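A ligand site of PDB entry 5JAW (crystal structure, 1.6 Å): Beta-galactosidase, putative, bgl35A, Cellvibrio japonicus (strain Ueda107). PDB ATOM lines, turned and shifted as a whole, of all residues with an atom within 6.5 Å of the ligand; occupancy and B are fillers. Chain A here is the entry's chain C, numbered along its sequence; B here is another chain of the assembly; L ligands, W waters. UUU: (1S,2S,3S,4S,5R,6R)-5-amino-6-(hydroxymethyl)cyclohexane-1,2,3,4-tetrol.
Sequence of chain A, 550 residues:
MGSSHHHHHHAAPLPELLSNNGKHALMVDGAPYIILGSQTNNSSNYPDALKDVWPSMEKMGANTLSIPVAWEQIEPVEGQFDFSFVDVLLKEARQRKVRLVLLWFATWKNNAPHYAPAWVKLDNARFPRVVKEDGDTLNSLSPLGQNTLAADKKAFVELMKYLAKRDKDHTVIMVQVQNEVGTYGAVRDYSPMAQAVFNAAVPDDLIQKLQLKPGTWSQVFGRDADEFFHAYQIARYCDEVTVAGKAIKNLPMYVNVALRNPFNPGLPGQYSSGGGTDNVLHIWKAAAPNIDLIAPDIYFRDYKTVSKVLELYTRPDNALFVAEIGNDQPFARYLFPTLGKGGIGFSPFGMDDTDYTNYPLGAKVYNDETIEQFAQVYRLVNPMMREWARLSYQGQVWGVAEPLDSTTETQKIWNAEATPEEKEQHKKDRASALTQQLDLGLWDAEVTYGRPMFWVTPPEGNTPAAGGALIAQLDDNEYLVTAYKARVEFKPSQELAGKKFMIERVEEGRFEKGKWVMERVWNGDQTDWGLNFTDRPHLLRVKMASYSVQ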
ATOM      1  N   GLN A  39      -5.462 -22.481  -7.466  1.00  0.00           N
ATOM      2  CA  GLN A  39      -5.288 -22.537  -8.870  1.00  0.00           C
ATOM      3  C   GLN A  39      -6.629 -22.726  -9.570  1.00  0.00           C
ATOM      4  O   GLN A  39      -7.379 -23.629  -9.192  1.00  0.00           O
ATOM      5  CB  GLN A  39      -4.221 -23.590  -9.250  1.00  0.00           C
ATOM      6  CG  GLN A  39      -3.928 -23.719 -10.729  1.00  0.00           C
ATOM      7  CD  GLN A  39      -2.746 -24.656 -11.167  1.00  0.00           C
ATOM      8  OE1 GLN A  39      -2.764 -25.115 -12.251  1.00  0.00           O
ATOM      9  NE2 GLN A  39      -1.751 -24.886 -10.304  1.00  0.00           N
ATOM     10  N   THR A  40      -6.794 -22.031 -10.686  1.00  0.00           N
ATOM     11  CA  THR A  40      -8.043 -22.176 -11.434  1.00  0.00           C
ATOM     12  C   THR A  40      -8.141 -23.494 -12.210  1.00  0.00           C
ATOM     13  O   THR A  40      -7.099 -24.079 -12.499  1.00  0.00           O
ATOM     14  CB  THR A  40      -8.193 -20.990 -12.454  1.00  0.00           C
ATOM     15  OG1 THR A  40      -7.287 -21.113 -13.522  1.00  0.00           O
ATOM     16  CG2 THR A  40      -8.080 -19.651 -11.746  1.00  0.00           C
ATOM     17  N   ASN A  41      -9.344 -23.940 -12.628  1.00  0.00           N
ATOM     18  CA  ASN A  41      -9.461 -24.844 -13.817  1.00  0.00           C
ATOM     19  C   ASN A  41      -8.828 -24.267 -15.067  1.00  0.00           C
ATOM     20  O   ASN A  41      -8.454 -23.136 -15.112  1.00  0.00           O
ATOM     21  CB  ASN A  41     -10.914 -25.345 -14.055  1.00  0.00           C
ATOM     22  CG  ASN A  41     -11.342 -26.270 -12.961  1.00  0.00           C
ATOM     23  OD1 ASN A  41     -10.800 -27.355 -12.816  1.00  0.00           O
ATOM     24  ND2 ASN A  41     -12.236 -25.793 -12.103  1.00  0.00           N
ATOM     25  N   ASN A  42      -8.568 -25.134 -16.044  1.00  0.00           N
ATOM     26  CA  ASN A  42      -7.764 -24.800 -17.235  1.00  0.00           C
ATOM     27  C   ASN A  42      -8.461 -23.853 -18.228  1.00  0.00           C
ATOM     28  O   ASN A  42      -7.774 -23.426 -19.214  1.00  0.00           O
ATOM     29  CB  ASN A  42      -7.436 -26.016 -18.014  1.00  0.00           C
ATOM     30  CG  ASN A  42      -6.399 -27.003 -17.362  1.00  0.00           C
ATOM     31  OD1 ASN A  42      -6.305 -28.144 -17.854  1.00  0.00           O
ATOM     32  ND2 ASN A  42      -5.577 -26.523 -16.330  1.00  0.00           N
ATOM     33  N   LEU A 103       0.669 -18.860 -15.339  1.00  0.00           N
ATOM     34  CA  LEU A 103       1.100 -20.104 -15.939  1.00  0.00           C
ATOM     35  C   LEU A 103       1.193 -20.062 -17.448  1.00  0.00           C
ATOM     36  O   LEU A 103       0.105 -19.949 -18.061  1.00  0.00           O
ATOM     37  CB  LEU A 103       0.197 -21.295 -15.522  1.00  0.00           C
ATOM     38  CG  LEU A 103      -0.301 -21.276 -14.084  1.00  0.00           C
ATOM     39  CD1 LEU A 103      -1.234 -22.398 -13.794  1.00  0.00           C
ATOM     40  CD2 LEU A 103       0.895 -21.507 -13.132  1.00  0.00           C
ATOM     41  N   PHE A 105       1.112 -21.251 -20.736  1.00  0.00           N
ATOM     42  CA  PHE A 105       0.689 -22.455 -21.464  1.00  0.00           C
ATOM     43  C   PHE A 105       1.059 -22.230 -22.934  1.00  0.00           C
ATOM     44  O   PHE A 105       0.422 -21.394 -23.574  1.00  0.00           O
ATOM     45  CB  PHE A 105      -0.815 -22.552 -21.343  1.00  0.00           C
ATOM     46  CG  PHE A 105      -1.358 -23.145 -20.048  1.00  0.00           C
ATOM     47  CD1 PHE A 105      -0.560 -23.468 -18.943  1.00  0.00           C
ATOM     48  CD2 PHE A 105      -2.716 -23.444 -19.974  1.00  0.00           C
ATOM     49  CE1 PHE A 105      -1.146 -24.050 -17.815  1.00  0.00           C
ATOM     50  CE2 PHE A 105      -3.281 -23.996 -18.848  1.00  0.00           C
ATOM     51  CZ  PHE A 105      -2.463 -24.317 -17.767  1.00  0.00           C
ATOM     52  N   LYS A 109       1.549 -28.006 -22.685  1.00  0.00           N
ATOM     53  CA  LYS A 109       0.618 -28.014 -21.620  1.00  0.00           C
ATOM     54  C   LYS A 109       0.210 -29.529 -21.471  1.00  0.00           C
ATOM     55  O   LYS A 109      -0.413 -30.080 -22.396  1.00  0.00           O
ATOM     56  CB  LYS A 109      -0.569 -27.120 -21.904  1.00  0.00           C
ATOM     57  CG  LYS A 109      -1.391 -26.915 -20.650  1.00  0.00           C
ATOM     58  CD  LYS A 109      -2.231 -28.113 -20.283  1.00  0.00           C
ATOM     59  CE  LYS A 109      -3.334 -27.849 -19.277  1.00  0.00           C
ATOM     60  NZ  LYS A 109      -3.888 -29.026 -18.573  1.00  0.00           N
ATOM     61  N   ASN A 110       0.636 -30.270 -20.383  1.00  0.00           N
ATOM     62  CA  ASN A 110       0.395 -31.666 -20.262  1.00  0.00           C
ATOM     63  C   ASN A 110       0.795 -32.402 -21.557  1.00  0.00           C
ATOM     64  O   ASN A 110       0.009 -33.176 -22.123  1.00  0.00           O
ATOM     65  CB  ASN A 110      -1.088 -31.954 -19.979  1.00  0.00           C
ATOM     66  CG  ASN A 110      -1.560 -31.482 -18.634  1.00  0.00           C
ATOM     67  OD1 ASN A 110      -1.160 -30.426 -18.103  1.00  0.00           O
ATOM     68  ND2 ASN A 110      -2.532 -32.198 -18.068  1.00  0.00           N
ATOM     69  N   GLN A 176       5.358 -19.659 -14.183  1.00  0.00           N
ATOM     70  CA  GLN A 176       5.597 -21.034 -14.605  1.00  0.00           C
ATOM     71  C   GLN A 176       5.783 -21.068 -16.069  1.00  0.00           C
ATOM     72  O   GLN A 176       4.928 -20.582 -16.827  1.00  0.00           O
ATOM     73  CB  GLN A 176       4.383 -21.950 -14.279  1.00  0.00           C
ATOM     74  CG  GLN A 176       4.590 -23.471 -14.299  1.00  0.00           C
ATOM     75  CD  GLN A 176       3.270 -24.221 -14.052  1.00  0.00           C
ATOM     76  OE1 GLN A 176       2.827 -24.497 -12.912  1.00  0.00           O
ATOM     77  NE2 GLN A 176       2.583 -24.494 -15.122  1.00  0.00           N
ATOM     78  N   ASN A 179       3.544 -25.905 -18.903  1.00  0.00           N
ATOM     79  CA  ASN A 179       2.853 -26.612 -17.905  1.00  0.00           C
ATOM     80  C   ASN A 179       3.031 -28.103 -18.129  1.00  0.00           C
ATOM     81  O   ASN A 179       2.617 -28.623 -19.154  1.00  0.00           O
ATOM     82  CB  ASN A 179       1.400 -26.234 -17.943  1.00  0.00           C
ATOM     83  CG  ASN A 179       0.612 -26.847 -16.841  1.00  0.00           C
ATOM     84  OD1 ASN A 179       0.556 -26.261 -15.750  1.00  0.00           O
ATOM     85  ND2 ASN A 179       0.086 -28.032 -17.061  1.00  0.00           N
ATOM     86  N   GLU A 180       3.605 -28.855 -17.199  1.00  0.00           N
ATOM     87  CA  GLU A 180       3.786 -30.276 -17.387  1.00  0.00           C
ATOM     88  C   GLU A 180       4.329 -30.704 -18.756  1.00  0.00           C
ATOM     89  O   GLU A 180       3.641 -31.310 -19.590  1.00  0.00           O
ATOM     90  CB  GLU A 180       2.494 -30.976 -16.966  1.00  0.00           C
ATOM     91  CG  GLU A 180       2.142 -30.931 -15.492  1.00  0.00           C
ATOM     92  CD  GLU A 180       1.157 -32.007 -14.963  1.00  0.00           C
ATOM     93  OE1 GLU A 180       0.481 -32.734 -15.732  1.00  0.00           O
ATOM     94  OE2 GLU A 180       1.011 -32.149 -13.747  1.00  0.00           O
ATOM     95  N   ASN A 256       6.752 -27.226 -13.563  1.00  0.00           N
ATOM     96  CA  ASN A 256       5.909 -28.108 -12.759  1.00  0.00           C
ATOM     97  C   ASN A 256       5.812 -29.528 -13.388  1.00  0.00           C
ATOM     98  O   ASN A 256       5.467 -29.682 -14.578  1.00  0.00           O
ATOM     99  CB  ASN A 256       4.495 -27.501 -12.538  1.00  0.00           C
ATOM    100  CG  ASN A 256       3.704 -27.326 -13.807  1.00  0.00           C
ATOM    101  OD1 ASN A 256       4.290 -26.894 -14.864  1.00  0.00           O
ATOM    102  ND2 ASN A 256       2.346 -27.596 -13.710  1.00  0.00           N
ATOM    103  N   ASP A 297       3.712 -31.725  -9.045  1.00  0.00           N
ATOM    104  CA  ASP A 297       2.262 -31.677  -9.135  1.00  0.00           C
ATOM    105  C   ASP A 297       1.736 -32.942  -8.466  1.00  0.00           C
ATOM    106  O   ASP A 297       2.040 -34.003  -8.981  1.00  0.00           O
ATOM    107  CB  ASP A 297       1.873 -31.620 -10.594  1.00  0.00           C
ATOM    108  CG  ASP A 297       2.087 -30.291 -11.189  1.00  0.00           C
ATOM    109  OD1 ASP A 297       2.434 -29.300 -10.487  1.00  0.00           O
ATOM    110  OD2 ASP A 297       1.959 -30.173 -12.416  1.00  0.00           O
ATOM    111  N   TYR A 299      -1.040 -35.509  -7.274  1.00  0.00           N
ATOM    112  CA  TYR A 299      -2.343 -36.095  -7.251  1.00  0.00           C
ATOM    113  C   TYR A 299      -2.440 -37.459  -6.569  1.00  0.00           C
ATOM    114  O   TYR A 299      -3.523 -38.006  -6.427  1.00  0.00           O
ATOM    115  CB  TYR A 299      -2.971 -36.041  -8.621  1.00  0.00           C
ATOM    116  CG  TYR A 299      -3.949 -34.887  -8.784  1.00  0.00           C
ATOM    117  CD1 TYR A 299      -5.160 -34.885  -8.160  1.00  0.00           C
ATOM    118  CD2 TYR A 299      -3.578 -33.748  -9.538  1.00  0.00           C
ATOM    119  CE1 TYR A 299      -6.062 -33.846  -8.339  1.00  0.00           C
ATOM    120  CE2 TYR A 299      -4.463 -32.670  -9.656  1.00  0.00           C
ATOM    121  CZ  TYR A 299      -5.681 -32.748  -9.059  1.00  0.00           C
ATOM    122  OH  TYR A 299      -6.566 -31.689  -9.199  1.00  0.00           O
ATOM    123  N   GLU A 324       0.755 -27.803  -7.712  1.00  0.00           N
ATOM    124  CA  GLU A 324      -0.576 -28.398  -8.002  1.00  0.00           C
ATOM    125  C   GLU A 324      -0.827 -29.453  -6.962  1.00  0.00           C
ATOM    126  O   GLU A 324       0.043 -30.283  -6.724  1.00  0.00           O
ATOM    127  CB  GLU A 324      -0.601 -29.025  -9.351  1.00  0.00           C
ATOM    128  CG  GLU A 324      -2.014 -29.481  -9.807  1.00  0.00           C
ATOM    129  CD  GLU A 324      -1.893 -30.554 -10.899  1.00  0.00           C
ATOM    130  OE1 GLU A 324      -2.377 -30.154 -12.127  1.00  0.00           O
ATOM    131  OE2 GLU A 324      -1.393 -31.672 -10.782  1.00  0.00           O
ATOM    132  N   PHE A 349      -5.688 -27.325  -6.898  1.00  0.00           N
ATOM    133  CA  PHE A 349      -6.136 -27.122  -8.279  1.00  0.00           C
ATOM    134  C   PHE A 349      -7.651 -27.177  -8.355  1.00  0.00           C
ATOM    135  O   PHE A 349      -8.303 -27.949  -7.666  1.00  0.00           O
ATOM    136  CB  PHE A 349      -5.593 -28.227  -9.100  1.00  0.00           C
ATOM    137  CG  PHE A 349      -5.914 -28.106 -10.574  1.00  0.00           C
ATOM    138  CD1 PHE A 349      -5.236 -27.233 -11.313  1.00  0.00           C
ATOM    139  CD2 PHE A 349      -7.042 -28.738 -11.107  1.00  0.00           C
ATOM    140  CE1 PHE A 349      -5.542 -27.033 -12.672  1.00  0.00           C
ATOM    141  CE2 PHE A 349      -7.323 -28.596 -12.468  1.00  0.00           C
ATOM    142  CZ  PHE A 349      -6.587 -27.730 -13.217  1.00  0.00           C
ATOM    143  N   TYR A 356     -16.698 -27.533 -13.624  1.00  0.00           N
ATOM    144  CA  TYR A 356     -15.859 -28.577 -14.027  1.00  0.00           C
ATOM    145  C   TYR A 356     -15.282 -29.174 -12.737  1.00  0.00           C
ATOM    146  O   TYR A 356     -14.886 -28.433 -11.830  1.00  0.00           O
ATOM    147  CB  TYR A 356     -14.713 -28.159 -14.921  1.00  0.00           C
ATOM    148  CG  TYR A 356     -13.866 -29.353 -15.380  1.00  0.00           C
ATOM    149  CD1 TYR A 356     -14.207 -30.059 -16.489  1.00  0.00           C
ATOM    150  CD2 TYR A 356     -12.701 -29.813 -14.705  1.00  0.00           C
ATOM    151  CE1 TYR A 356     -13.519 -31.131 -16.942  1.00  0.00           C
ATOM    152  CE2 TYR A 356     -11.990 -30.863 -15.191  1.00  0.00           C
ATOM    153  CZ  TYR A 356     -12.375 -31.541 -16.273  1.00  0.00           C
ATOM    154  OH  TYR A 356     -11.625 -32.550 -16.700  1.00  0.00           O
ATOM    155  N   ASN A 358     -12.394 -32.442 -11.907  1.00  0.00           N
ATOM    156  CA  ASN A 358     -11.542 -33.465 -12.456  1.00  0.00           C
ATOM    157  C   ASN A 358     -11.598 -34.839 -11.629  1.00  0.00           C
ATOM    158  O   ASN A 358     -10.752 -35.685 -11.798  1.00  0.00           O
ATOM    159  CB  ASN A 358     -10.062 -32.998 -12.585  1.00  0.00           C
ATOM    160  CG  ASN A 358      -9.470 -32.643 -11.227  1.00  0.00           C
ATOM    161  OD1 ASN A 358     -10.119 -32.828 -10.176  1.00  0.00           O
ATOM    162  ND2 ASN A 358      -8.294 -32.074 -11.224  1.00  0.00           N
ATOM    163  N   LEU A 361      -9.733 -37.450  -9.685  1.00  0.00           N
ATOM    164  CA  LEU A 361      -8.540 -36.796  -9.158  1.00  0.00           C
ATOM    165  C   LEU A 361      -8.882 -35.864  -8.006  1.00  0.00           C
ATOM    166  O   LEU A 361      -8.330 -36.029  -6.895  1.00  0.00           O
ATOM    167  CB  LEU A 361      -7.846 -36.037 -10.281  1.00  0.00           C
ATOM    168  CG  LEU A 361      -7.313 -36.950 -11.347  1.00  0.00           C
ATOM    169  CD1 LEU A 361      -6.796 -36.120 -12.494  1.00  0.00           C
ATOM    170  CD2 LEU A 361      -6.267 -37.905 -10.776  1.00  0.00           C
ATOM    171  N   PHE B 454     -13.468 -36.260 -16.468  1.00  0.00           N
ATOM    172  CA  PHE B 454     -12.047 -36.528 -16.611  1.00  0.00           C
ATOM    173  C   PHE B 454     -11.773 -38.014 -16.807  1.00  0.00           C
ATOM    174  O   PHE B 454     -12.428 -38.875 -16.155  1.00  0.00           O
ATOM    175  CB  PHE B 454     -11.311 -36.065 -15.301  1.00  0.00           C
ATOM    176  CG  PHE B 454      -9.841 -36.039 -15.437  1.00  0.00           C
ATOM    177  CD1 PHE B 454      -9.068 -37.194 -15.300  1.00  0.00           C
ATOM    178  CD2 PHE B 454      -9.220 -34.824 -15.684  1.00  0.00           C
ATOM    179  CE1 PHE B 454      -7.667 -37.131 -15.484  1.00  0.00           C
ATOM    180  CE2 PHE B 454      -7.857 -34.734 -15.827  1.00  0.00           C
ATOM    181  CZ  PHE B 454      -7.079 -35.887 -15.732  1.00  0.00           C
ATOM    182  N   GLY B 524      -7.420 -27.676 -22.675  1.00  0.00           N
ATOM    183  CA  GLY B 524      -6.860 -28.451 -21.569  1.00  0.00           C
ATOM    184  C   GLY B 524      -7.754 -29.523 -21.080  1.00  0.00           C
ATOM    185  O   GLY B 524      -8.376 -30.266 -21.849  1.00  0.00           O
ATOM    186  N   ASP B 525      -7.947 -29.597 -19.751  1.00  0.00           N
ATOM    187  CA  ASP B 525      -8.787 -30.578 -19.109  1.00  0.00           C
ATOM    188  C   ASP B 525     -10.202 -30.562 -19.724  1.00  0.00           C
ATOM    189  O   ASP B 525     -10.851 -31.605 -19.783  1.00  0.00           O
ATOM    190  CB  ASP B 525      -8.964 -30.313 -17.614  1.00  0.00           C
ATOM    191  CG  ASP B 525      -7.695 -30.509 -16.794  1.00  0.00           C
ATOM    192  OD1 ASP B 525      -6.771 -31.179 -17.184  1.00  0.00           O
ATOM    193  OD2 ASP B 525      -7.785 -30.015 -15.686  1.00  0.00           O
ATOM    194  N   ASP B 528      -9.740 -32.463 -23.188  1.00  0.00           N
ATOM    195  CA  ASP B 528      -8.929 -33.672 -23.307  1.00  0.00           C
ATOM    196  C   ASP B 528      -9.752 -34.935 -23.280  1.00  0.00           C
ATOM    197  O   ASP B 528      -9.265 -35.926 -23.861  1.00  0.00           O
ATOM    198  CB  ASP B 528      -7.951 -33.786 -22.168  1.00  0.00           C
ATOM    199  CG  ASP B 528      -6.795 -32.855 -22.291  1.00  0.00           C
ATOM    200  OD1 ASP B 528      -6.308 -32.538 -23.412  1.00  0.00           O
ATOM    201  OD2 ASP B 528      -6.271 -32.631 -21.211  1.00  0.00           O
HETATM  202  C1  UUU L   1      -4.534 -30.213 -14.771  1.00  0.00           C
HETATM  203  C2  UUU L   1      -4.634 -31.232 -13.596  1.00  0.00           C
HETATM  204  C3  UUU L   1      -3.233 -31.875 -13.393  1.00  0.00           C
HETATM  205  C4  UUU L   1      -2.123 -30.850 -13.220  1.00  0.00           C
HETATM  206  C5  UUU L   1      -2.054 -29.922 -14.441  1.00  0.00           C
HETATM  207  C6  UUU L   1      -3.413 -29.208 -14.540  1.00  0.00           C
HETATM  208  C8  UUU L   1      -5.658 -32.273 -13.823  1.00  0.00           C
HETATM  209  O8  UUU L   1      -6.960 -31.729 -13.690  1.00  0.00           O
HETATM  210  O1  UUU L   1      -4.363 -30.841 -16.044  1.00  0.00           O
HETATM  211  O6  UUU L   1      -3.301 -28.259 -15.627  1.00  0.00           O
HETATM  212  O5  UUU L   1      -0.968 -29.026 -14.410  1.00  0.00           O
HETATM  213  N1  UUU L   1      -2.868 -32.806 -14.439  1.00  0.00           N
HETATM  214  O   HOH W   1      -2.083 -26.023 -14.880  1.00  0.00           O
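O5 of the ligand sits at hydrogen-bond distance from ND2 of Asn 179, at 3.0 Å. The side-chain amide nitrogen (ND2) of Asn 358 lies within hydrogen-bond range of an oxygen (O8) of the ligand (2.8 Å). ND2 of Asn 42 is in hydrogen-bond range of O6 of the ligand, at 2.9 Å. ND2 of Asn 110 lies within hydrogen-bond range of O1 of the ligand. An oxygen (O6) of the ligand is in hydrogen-bond range of the side-chain amino group (NZ) of Lys 109, 3.1 Å away. The side-chain carboxylate (OE1) of Glu 180 is in salt-bridge range of a nitrogen (N1) of the ligand (3.6 Å). The side-chain carboxylate (OD1) of Asp 525 of chain B lies within hydrogen-bond range of an oxygen (O1) of the ligand, at 2.7 Å. OE1 of Glu 324 is bonded to C4 of the ligand (1.3 Å).
OD2 of Asp 297 lies within hydrogen-bond range of ND2 of Asn 256, at 2.9 Å. O of Asp 525 of chain B lies within hydrogen-bond range of OH of Tyr 356, 3.3 Å away. OD1 of Asn 256 sits at hydrogen-bond distance from NE2 of Gln 176 (3.0 Å). The side-chain amide nitrogen (ND2) of Asn 358 is in hydrogen-bond range of the side-chain hydroxyl (OH) of Tyr 299. NZ of Lys 109 lies within hydrogen-bond range of OD1 of Asn 42 (2.7 Å). OD1 of Asn 42 sits at hydrogen-bond distance from N of Asp 525 of chain B (2.9 Å). The backbone NH of Asn 110 sits at hydrogen-bond distance from the backbone carbonyl oxygen of Glu 180, at 3.3 Å. N of Glu 180 is in hydrogen-bond range of OD1 of Asn 256 (3.1 Å).
Residues that only touch the ligand: Phe 349 (3.4 Å), Asn 256 (3.7 Å), Asp 297 (3.7 Å) and Phe 454 of chain B (3.8 Å). Of the 23 residues printed, 12 come within 4 Å of the ligand. The nearest printed residue that does not touch the ligand is Tyr 299 (4.01 Å).
Water W1 lies within hydrogen-bond range of an oxygen (O6) of the ligand, the side-chain amide oxygen of Asn 179 and the side-chain amide oxygen of Gln 39.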
